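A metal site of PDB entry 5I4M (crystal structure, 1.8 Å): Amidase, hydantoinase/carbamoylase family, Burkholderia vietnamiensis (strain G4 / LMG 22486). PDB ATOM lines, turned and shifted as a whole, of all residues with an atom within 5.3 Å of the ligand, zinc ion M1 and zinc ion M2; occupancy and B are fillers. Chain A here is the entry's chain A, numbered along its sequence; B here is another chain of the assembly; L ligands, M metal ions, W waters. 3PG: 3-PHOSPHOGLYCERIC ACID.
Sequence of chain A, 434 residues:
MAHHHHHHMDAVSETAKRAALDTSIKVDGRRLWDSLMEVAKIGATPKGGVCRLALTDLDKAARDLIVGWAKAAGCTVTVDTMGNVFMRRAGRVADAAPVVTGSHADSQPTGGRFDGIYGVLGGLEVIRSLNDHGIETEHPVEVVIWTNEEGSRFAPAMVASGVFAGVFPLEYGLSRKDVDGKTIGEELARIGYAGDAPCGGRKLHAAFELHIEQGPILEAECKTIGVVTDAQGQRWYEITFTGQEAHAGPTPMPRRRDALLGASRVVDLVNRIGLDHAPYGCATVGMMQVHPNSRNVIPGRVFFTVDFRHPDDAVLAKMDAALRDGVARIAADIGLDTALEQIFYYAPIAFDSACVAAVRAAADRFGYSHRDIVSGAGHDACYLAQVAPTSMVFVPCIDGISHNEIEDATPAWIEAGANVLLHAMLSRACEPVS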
ATOM      1  N   SER A 103      32.436  16.969 -19.193  1.00  0.00           N
ATOM      2  CA  SER A 103      31.707  18.228 -19.196  1.00  0.00           C
ATOM      3  C   SER A 103      32.203  19.034 -18.004  1.00  0.00           C
ATOM      4  O   SER A 103      33.369  18.939 -17.628  1.00  0.00           O
ATOM      5  CB  SER A 103      30.195  17.940 -19.146  1.00  0.00           C
ATOM      6  OG  SER A 103      29.410  19.054 -19.602  1.00  0.00           O
ATOM      7  N   HIS A 104      31.326  19.821 -17.383  1.00  0.00           N
ATOM      8  CA  HIS A 104      31.728  20.673 -16.279  1.00  0.00           C
ATOM      9  C   HIS A 104      30.897  20.388 -15.047  1.00  0.00           C
ATOM     10  O   HIS A 104      29.705  20.063 -15.134  1.00  0.00           O
ATOM     11  CB  HIS A 104      31.615  22.156 -16.651  1.00  0.00           C
ATOM     12  CG  HIS A 104      30.251  22.558 -17.116  1.00  0.00           C
ATOM     13  ND1 HIS A 104      29.356  23.216 -16.298  1.00  0.00           N
ATOM     14  CD2 HIS A 104      29.637  22.423 -18.311  1.00  0.00           C
ATOM     15  CE1 HIS A 104      28.242  23.457 -16.970  1.00  0.00           C
ATOM     16  NE2 HIS A 104      28.391  22.990 -18.195  1.00  0.00           N
ATOM     17  N   GLN A 108      26.104  28.012 -12.753  1.00  0.00           N
ATOM     18  CA  GLN A 108      25.704  29.388 -12.590  1.00  0.00           C
ATOM     19  C   GLN A 108      25.204  29.612 -11.160  1.00  0.00           C
ATOM     20  O   GLN A 108      24.883  28.652 -10.457  1.00  0.00           O
ATOM     21  CB  GLN A 108      24.592  29.721 -13.580  1.00  0.00           C
ATOM     22  CG  GLN A 108      25.045  29.633 -14.997  1.00  0.00           C
ATOM     23  CD  GLN A 108      25.807  30.880 -15.386  1.00  0.00           C
ATOM     24  OE1 GLN A 108      25.633  31.924 -14.759  1.00  0.00           O
ATOM     25  NE2 GLN A 108      26.665  30.774 -16.400  1.00  0.00           N
ATOM     26  N   ASP A 115      22.784  20.943 -16.031  1.00  0.00           N
ATOM     27  CA  ASP A 115      23.733  21.599 -16.936  1.00  0.00           C
ATOM     28  C   ASP A 115      25.152  21.221 -16.535  1.00  0.00           C
ATOM     29  O   ASP A 115      25.543  21.390 -15.369  1.00  0.00           O
ATOM     30  CB  ASP A 115      23.504  23.117 -16.880  1.00  0.00           C
ATOM     31  CG  ASP A 115      24.487  23.922 -17.708  1.00  0.00           C
ATOM     32  OD1 ASP A 115      25.292  23.362 -18.481  1.00  0.00           O
ATOM     33  OD2 ASP A 115      24.394  25.182 -17.608  1.00  0.00           O
ATOM     34  N   GLY A 116      25.895  20.639 -17.472  1.00  0.00           N
ATOM     35  CA  GLY A 116      27.249  20.205 -17.196  1.00  0.00           C
ATOM     36  C   GLY A 116      27.396  18.923 -16.395  1.00  0.00           C
ATOM     37  O   GLY A 116      28.064  17.987 -16.827  1.00  0.00           O
ATOM     38  N   GLU A 149      33.811  26.115 -16.750  1.00  0.00           N
ATOM     39  CA  GLU A 149      33.249  26.154 -18.087  1.00  0.00           C
ATOM     40  C   GLU A 149      32.243  27.297 -18.241  1.00  0.00           C
ATOM     41  O   GLU A 149      32.116  27.841 -19.339  1.00  0.00           O
ATOM     42  CB  GLU A 149      32.606  24.805 -18.452  1.00  0.00           C
ATOM     43  CG  GLU A 149      32.070  24.704 -19.882  1.00  0.00           C
ATOM     44  CD  GLU A 149      30.668  25.287 -20.045  1.00  0.00           C
ATOM     45  OE1 GLU A 149      30.025  25.591 -19.022  1.00  0.00           O
ATOM     46  OE2 GLU A 149      30.231  25.441 -21.198  1.00  0.00           O
ATOM     47  N   GLU A 150      31.554  27.690 -17.162  1.00  0.00           N
ATOM     48  CA  GLU A 150      30.421  28.602 -17.321  1.00  0.00           C
ATOM     49  C   GLU A 150      30.875  30.013 -17.690  1.00  0.00           C
ATOM     50  O   GLU A 150      30.109  30.761 -18.316  1.00  0.00           O
ATOM     51  CB  GLU A 150      29.572  28.659 -16.059  1.00  0.00           C
ATOM     52  CG  GLU A 150      28.713  27.417 -15.791  1.00  0.00           C
ATOM     53  CD  GLU A 150      27.463  27.349 -16.661  1.00  0.00           C
ATOM     54  OE1 GLU A 150      27.313  28.179 -17.573  1.00  0.00           O
ATOM     55  OE2 GLU A 150      26.611  26.459 -16.430  1.00  0.00           O
ATOM     56  N   ALA A 157      33.821  32.028 -20.876  1.00  0.00           N
ATOM     57  CA  ALA A 157      33.502  30.613 -20.761  1.00  0.00           C
ATOM     58  C   ALA A 157      34.569  29.743 -21.421  1.00  0.00           C
ATOM     59  O   ALA A 157      35.348  30.196 -22.252  1.00  0.00           O
ATOM     60  CB  ALA A 157      32.152  30.324 -21.403  1.00  0.00           C
ATOM     61  N   MET A 158      34.578  28.470 -21.021  1.00  0.00           N
ATOM     62  CA  MET A 158      35.282  27.416 -21.742  1.00  0.00           C
ATOM     63  C   MET A 158      36.794  27.654 -21.808  1.00  0.00           C
ATOM     64  O   MET A 158      37.464  27.180 -22.733  1.00  0.00           O
ATOM     65  CB  MET A 158      34.707  27.259 -23.151  1.00  0.00           C
ATOM     66  CG  MET A 158      33.225  26.862 -23.165  1.00  0.00           C
ATOM     67  SD  MET A 158      32.312  27.609 -24.543  1.00  0.00           S
ATOM     68  CE  MET A 158      33.287  27.069 -25.941  1.00  0.00           C
ATOM     69  N   HIS A 211      24.895  16.384 -23.012  1.00  0.00           N
ATOM     70  CA  HIS A 211      24.437  17.621 -22.364  1.00  0.00           C
ATOM     71  C   HIS A 211      22.938  17.775 -22.567  1.00  0.00           C
ATOM     72  O   HIS A 211      22.377  17.268 -23.549  1.00  0.00           O
ATOM     73  CB  HIS A 211      25.159  18.831 -22.964  1.00  0.00           C
ATOM     74  CG  HIS A 211      25.266  19.997 -22.034  1.00  0.00           C
ATOM     75  ND1 HIS A 211      24.198  20.819 -21.735  1.00  0.00           N
ATOM     76  CD2 HIS A 211      26.327  20.509 -21.364  1.00  0.00           C
ATOM     77  CE1 HIS A 211      24.599  21.777 -20.917  1.00  0.00           C
ATOM     78  NE2 HIS A 211      25.887  21.610 -20.679  1.00  0.00           N
ATOM     79  N   GLN A 214      19.155  22.698 -23.264  1.00  0.00           N
ATOM     80  CA  GLN A 214      19.066  24.059 -22.751  1.00  0.00           C
ATOM     81  C   GLN A 214      18.151  24.944 -23.602  1.00  0.00           C
ATOM     82  O   GLN A 214      18.179  26.168 -23.482  1.00  0.00           O
ATOM     83  CB  GLN A 214      20.448  24.711 -22.604  1.00  0.00           C
ATOM     84  CG  GLN A 214      21.364  23.874 -21.715  1.00  0.00           C
ATOM     85  CD  GLN A 214      22.733  24.488 -21.586  1.00  0.00           C
ATOM     86  OE1 GLN A 214      23.503  24.467 -22.552  1.00  0.00           O
ATOM     87  NE2 GLN A 214      23.049  25.026 -20.413  1.00  0.00           N
ATOM     88  N   GLN A 234      29.869  32.645 -30.812  1.00  0.00           N
ATOM     89  CA  GLN A 234      29.597  33.633 -29.776  1.00  0.00           C
ATOM     90  C   GLN A 234      30.634  34.746 -29.807  1.00  0.00           C
ATOM     91  O   GLN A 234      31.789  34.532 -30.175  1.00  0.00           O
ATOM     92  CB  GLN A 234      29.606  33.012 -28.381  1.00  0.00           C
ATOM     93  CG  GLN A 234      28.730  31.786 -28.206  1.00  0.00           C
ATOM     94  CD  GLN A 234      28.438  31.501 -26.742  1.00  0.00           C
ATOM     95  OE1 GLN A 234      28.013  32.393 -26.014  1.00  0.00           O
ATOM     96  NE2 GLN A 234      28.684  30.274 -26.305  1.00  0.00           N
ATOM     97  N   TRP A 236      31.498  37.769 -26.808  1.00  0.00           N
ATOM     98  CA  TRP A 236      31.196  38.399 -25.528  1.00  0.00           C
ATOM     99  C   TRP A 236      32.010  39.680 -25.375  1.00  0.00           C
ATOM    100  O   TRP A 236      33.153  39.765 -25.818  1.00  0.00           O
ATOM    101  CB  TRP A 236      31.524  37.489 -24.340  1.00  0.00           C
ATOM    102  CG  TRP A 236      30.714  36.229 -24.227  1.00  0.00           C
ATOM    103  CD1 TRP A 236      29.876  35.686 -25.154  1.00  0.00           C
ATOM    104  CD2 TRP A 236      30.683  35.363 -23.089  1.00  0.00           C
ATOM    105  NE1 TRP A 236      29.315  34.519 -24.658  1.00  0.00           N
ATOM    106  CE2 TRP A 236      29.809  34.302 -23.399  1.00  0.00           C
ATOM    107  CE3 TRP A 236      31.324  35.377 -21.838  1.00  0.00           C
ATOM    108  CZ2 TRP A 236      29.542  33.259 -22.496  1.00  0.00           C
ATOM    109  CZ3 TRP A 236      31.060  34.363 -20.943  1.00  0.00           C
ATOM    110  CH2 TRP A 236      30.174  33.310 -21.270  1.00  0.00           C
ATOM    111  N   ASP A 307      26.416  39.771 -24.669  1.00  0.00           N
ATOM    112  CA  ASP A 307      26.476  38.372 -25.083  1.00  0.00           C
ATOM    113  C   ASP A 307      25.764  38.294 -26.428  1.00  0.00           C
ATOM    114  O   ASP A 307      24.561  38.569 -26.503  1.00  0.00           O
ATOM    115  CB  ASP A 307      25.804  37.485 -24.036  1.00  0.00           C
ATOM    116  CG  ASP A 307      25.824  35.991 -24.382  1.00  0.00           C
ATOM    117  OD1 ASP A 307      25.390  35.594 -25.471  1.00  0.00           O
ATOM    118  OD2 ASP A 307      26.266  35.222 -23.501  1.00  0.00           O
ATOM    119  N   ARG A 309      25.248  35.822 -30.003  1.00  0.00           N
ATOM    120  CA  ARG A 309      25.441  34.492 -30.595  1.00  0.00           C
ATOM    121  C   ARG A 309      24.680  34.411 -31.911  1.00  0.00           C
ATOM    122  O   ARG A 309      23.604  35.000 -32.061  1.00  0.00           O
ATOM    123  CB  ARG A 309      24.933  33.384 -29.658  1.00  0.00           C
ATOM    124  CG  ARG A 309      25.262  33.652 -28.199  1.00  0.00           C
ATOM    125  CD  ARG A 309      24.821  32.510 -27.303  1.00  0.00           C
ATOM    126  NE  ARG A 309      25.120  32.863 -25.918  1.00  0.00           N
ATOM    127  CZ  ARG A 309      25.373  31.983 -24.967  1.00  0.00           C
ATOM    128  NH1 ARG A 309      25.346  30.681 -25.235  1.00  0.00           N
ATOM    129  NH2 ARG A 309      25.694  32.400 -23.746  1.00  0.00           N
ATOM    130  N   TYR A 346      34.375  32.860 -30.660  1.00  0.00           N
ATOM    131  CA  TYR A 346      34.699  31.702 -31.487  1.00  0.00           C
ATOM    132  C   TYR A 346      33.652  31.555 -32.579  1.00  0.00           C
ATOM    133  O   TYR A 346      32.470  31.869 -32.371  1.00  0.00           O
ATOM    134  CB  TYR A 346      34.818  30.405 -30.667  1.00  0.00           C
ATOM    135  CG  TYR A 346      33.561  29.922 -29.978  1.00  0.00           C
ATOM    136  CD1 TYR A 346      32.689  29.045 -30.625  1.00  0.00           C
ATOM    137  CD2 TYR A 346      33.273  30.287 -28.663  1.00  0.00           C
ATOM    138  CE1 TYR A 346      31.540  28.569 -29.994  1.00  0.00           C
ATOM    139  CE2 TYR A 346      32.133  29.822 -28.027  1.00  0.00           C
ATOM    140  CZ  TYR A 346      31.273  28.981 -28.690  1.00  0.00           C
ATOM    141  OH  TYR A 346      30.152  28.523 -28.042  1.00  0.00           O
ATOM    142  N   GLY A 376      22.953  25.781 -29.003  1.00  0.00           N
ATOM    143  CA  GLY A 376      22.837  27.214 -28.827  1.00  0.00           C
ATOM    144  C   GLY A 376      23.779  27.721 -27.762  1.00  0.00           C
ATOM    145  O   GLY A 376      24.118  28.908 -27.719  1.00  0.00           O
ATOM    146  N   ALA A 377      24.206  26.825 -26.869  1.00  0.00           N
ATOM    147  CA  ALA A 377      25.203  27.154 -25.864  1.00  0.00           C
ATOM    148  C   ALA A 377      26.583  26.726 -26.337  1.00  0.00           C
ATOM    149  O   ALA A 377      26.730  25.960 -27.290  1.00  0.00           O
ATOM    150  CB  ALA A 377      24.874  26.481 -24.529  1.00  0.00           C
ATOM    151  N   GLY A 378      27.591  27.245 -25.656  1.00  0.00           N
ATOM    152  CA  GLY A 378      28.945  26.748 -25.818  1.00  0.00           C
ATOM    153  C   GLY A 378      29.203  25.591 -24.871  1.00  0.00           C
ATOM    154  O   GLY A 378      28.593  25.497 -23.797  1.00  0.00           O
ATOM    155  N   HIS A 379      30.098  24.703 -25.274  1.00  0.00           N
ATOM    156  CA  HIS A 379      30.491  23.563 -24.476  1.00  0.00           C
ATOM    157  C   HIS A 379      31.972  23.336 -24.657  1.00  0.00           C
ATOM    158  O   HIS A 379      32.560  23.746 -25.657  1.00  0.00           O
ATOM    159  CB  HIS A 379      29.714  22.312 -24.871  1.00  0.00           C
ATOM    160  CG  HIS A 379      28.246  22.537 -24.924  1.00  0.00           C
ATOM    161  ND1 HIS A 379      27.463  22.551 -23.788  1.00  0.00           N
ATOM    162  CD2 HIS A 379      27.413  22.796 -25.961  1.00  0.00           C
ATOM    163  CE1 HIS A 379      26.216  22.796 -24.127  1.00  0.00           C
ATOM    164  NE2 HIS A 379      26.154  22.944 -25.430  1.00  0.00           N
ATOM    165  N   SER A 402      17.142  26.570 -18.902  1.00  0.00           N
ATOM    166  CA  SER A 402      18.421  26.311 -18.265  1.00  0.00           C
ATOM    167  C   SER A 402      18.912  27.636 -17.706  1.00  0.00           C
ATOM    168  O   SER A 402      18.367  28.699 -18.018  1.00  0.00           O
ATOM    169  CB  SER A 402      19.426  25.693 -19.237  1.00  0.00           C
ATOM    170  OG  SER A 402      20.628  25.361 -18.583  1.00  0.00           O
ATOM    171  N   HIS A 403      19.925  27.566 -16.856  1.00  0.00           N
ATOM    172  CA  HIS A 403      20.426  28.722 -16.105  1.00  0.00           C
ATOM    173  C   HIS A 403      19.342  29.315 -15.215  1.00  0.00           C
ATOM    174  O   HIS A 403      19.351  30.511 -14.911  1.00  0.00           O
ATOM    175  CB  HIS A 403      21.051  29.758 -17.041  1.00  0.00           C
ATOM    176  CG  HIS A 403      22.400  29.326 -17.557  1.00  0.00           C
ATOM    177  ND1 HIS A 403      23.266  30.175 -18.216  1.00  0.00           N
ATOM    178  CD2 HIS A 403      23.018  28.122 -17.484  1.00  0.00           C
ATOM    179  CE1 HIS A 403      24.362  29.515 -18.523  1.00  0.00           C
ATOM    180  NE2 HIS A 403      24.245  28.269 -18.089  1.00  0.00           N
ATOM    181  N   HIS B 247      18.741  30.954 -19.924  1.00  0.00           N
ATOM    182  CA  HIS B 247      20.027  30.949 -20.610  1.00  0.00           C
ATOM    183  C   HIS B 247      20.105  32.100 -21.620  1.00  0.00           C
ATOM    184  O   HIS B 247      19.171  32.347 -22.385  1.00  0.00           O
ATOM    185  CB  HIS B 247      20.236  29.620 -21.342  1.00  0.00           C
ATOM    186  CG  HIS B 247      21.668  29.283 -21.530  1.00  0.00           C
ATOM    187  ND1 HIS B 247      22.511  30.021 -22.328  1.00  0.00           N
ATOM    188  CD2 HIS B 247      22.438  28.303 -20.987  1.00  0.00           C
ATOM    189  CE1 HIS B 247      23.732  29.508 -22.283  1.00  0.00           C
ATOM    190  NE2 HIS B 247      23.707  28.461 -21.477  1.00  0.00           N
ATOM    191  N   ASN B 296      26.014  35.409 -18.740  1.00  0.00           N
ATOM    192  CA  ASN B 296      25.279  34.523 -19.630  1.00  0.00           C
ATOM    193  C   ASN B 296      23.974  34.012 -19.008  1.00  0.00           C
ATOM    194  O   ASN B 296      23.514  32.917 -19.328  1.00  0.00           O
ATOM    195  CB  ASN B 296      26.163  33.366 -20.157  1.00  0.00           C
ATOM    196  CG  ASN B 296      26.944  32.623 -19.070  1.00  0.00           C
ATOM    197  OD1 ASN B 296      27.083  33.067 -17.934  1.00  0.00           O
ATOM    198  ND2 ASN B 296      27.506  31.466 -19.458  1.00  0.00           N
HETATM  199  C1  3PG L   1      27.422  29.535 -22.635  1.00  0.00           C
HETATM  200  O1  3PG L   1      26.876  30.493 -22.060  1.00  0.00           O
HETATM  201  O2  3PG L   1      26.985  29.059 -23.710  1.00  0.00           O
HETATM  202  C2  3PG L   1      28.656  28.947 -22.012  1.00  0.00           C
HETATM  203  O3  3PG L   1      29.417  28.221 -22.998  1.00  0.00           O
HETATM  204  C3  3PG L   1      28.223  27.997 -20.919  1.00  0.00           C
HETATM  205  O1P 3PG L   1      27.510  26.902 -21.502  1.00  0.00           O
HETATM  206  P   3PG L   1      26.595  25.939 -20.541  1.00  0.00           P
HETATM  207  O2P 3PG L   1      27.433  25.633 -19.323  1.00  0.00           O
HETATM  208  O3P 3PG L   1      25.387  26.798 -20.211  1.00  0.00           O
HETATM  209  O4P 3PG L   1      26.330  24.705 -21.427  1.00  0.00           O
HETATM  210 ZN    ZN M   1      26.964  23.370 -19.793  1.00  0.00          ZN
HETATM  211 ZN    ZN M   2      25.636  26.645 -18.235  1.00  0.00          ZN
HETATM  212  O   HOH W   1      28.575  23.008 -21.232  1.00  0.00           O
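Gly 116 touches zinc ion M1. OE1 of Glu 149 touches zinc ion M1, at 3.9 Å. Five residues have an atom within 4 Å of zinc ion M1: His 104, Asp 115, Gly 116, Glu 149 and His 211.
Zinc ion M1 is bound by OD1 of Asp 115 (2.1 Å), NE2 of His 104 (2.2 Å), water W1 (2.2 Å), O4P of the ligand (2.2 Å), NE2 of His 211 (2.2 Å) and O2P of the ligand (2.4 Å). Zinc ion M1 has six donor atoms within binding distance.
Zinc ion M2 is bound by O3P of the ligand (2.0 Å). OD2 of Asp 115 binds zinc ion M2, at 2.0 Å. Zinc ion M2 is bound by the side-chain carboxylate (OE2) of Glu 150 (2.1 Å). A ring nitrogen (NE2) of His 403 is bound to zinc ion M2 (2.1 Å). Zinc ion M2 is bound by an oxygen (O2P) of the ligand. OE1 of Glu 150 binds zinc ion M2 (2.4 Å).
Ala 157 touches the ligand (CB to O3, 3.8 Å). Trp 236 touches the ligand (CZ2 to O1, 3.9 Å). Ala 377 touches the ligand (CA to O2, 3.4 Å). Hydrophobic or aromatic side chains within 4 Å of the ligand: His 104, Ala 157, Met 158, His 211, Trp 236, Ala 377, His 379, His 403 and His 247 of chain B. Along chain A the residues within 4 Å of the ligand span positions 104 to 403.
Merely in contact with zinc ion M2: Gln 214 (3.7 Å). The nearest printed residue that does not touch zinc ion M2 is His 247 of chain B (4.2 Å).
Water W1 lies within hydrogen-bond range of a ring nitrogen (ND1) of His 379 (2.8 Å) and the side-chain carboxylate (OE2) of Glu 149 (2.9 Å).
O3 of the ligand lies close to OE2 of Glu 149, 3.4 Å away. A ring nitrogen (NE2) of His 247 of chain B lies close to an oxygen (O3P) of the ligand (2.7 Å). N of Gly 378 sits at hydrogen-bond distance from O2 of the ligand (2.7 Å). O of Gly 378 lies within hydrogen-bond range of O3 of the ligand, 3.0 Å away. The guanidinium group (NH1) of Arg 309 lies within salt-bridge range of an oxygen (O2) of the ligand, 2.8 Å away. ND2 of Asn 296 of chain B lies within hydrogen-bond range of O1 of the ligand, 2.8 Å away. The side-chain amide nitrogen (NE2) of Gln 214 sits close to an oxygen (O3P) of the ligand (2.9 Å). An oxygen (O4P) of the ligand sits close to a ring nitrogen (ND1) of His 379, at 3.4 Å. The side-chain amide nitrogen of Gln 234 is in hydrogen-bond range of an oxygen (O2) of the ligand, 3.3 Å away. An oxygen (O3) of the ligand sits at hydrogen-bond distance from the side-chain sulfur of Met 158.
The side-chain carboxylate (OD2) of Asp 115 lies close to the side-chain amide nitrogen (NE2) of Gln 214, at 3.1 Å. The side-chain amide nitrogen of Asn 296 of chain B sits at hydrogen-bond distance from the backbone carbonyl oxygen of Glu 150 (2.9 Å). The backbone carbonyl oxygen (O) of Asn 296 of chain B is in hydrogen-bond range of a ring nitrogen (ND1) of His 403, at 3.0 Å. NE of Arg 309 lies close to OE1 of Gln 234 (2.9 Å). The guanidinium group (NH1) of Arg 309 is in hydrogen-bond range of the backbone carbonyl oxygen (O) of Gly 376 (3.3 Å). OD1 of Asp 307 is in salt-bridge range of NE of Arg 309 (2.8 Å). OG of Ser 402 is in hydrogen-bond range of NE2 of Gln 214, 3.1 Å away. The side-chain amide oxygen (OE1) of Gln 234 sits at hydrogen-bond distance from the indole nitrogen (NE1) of Trp 236 (2.8 Å).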
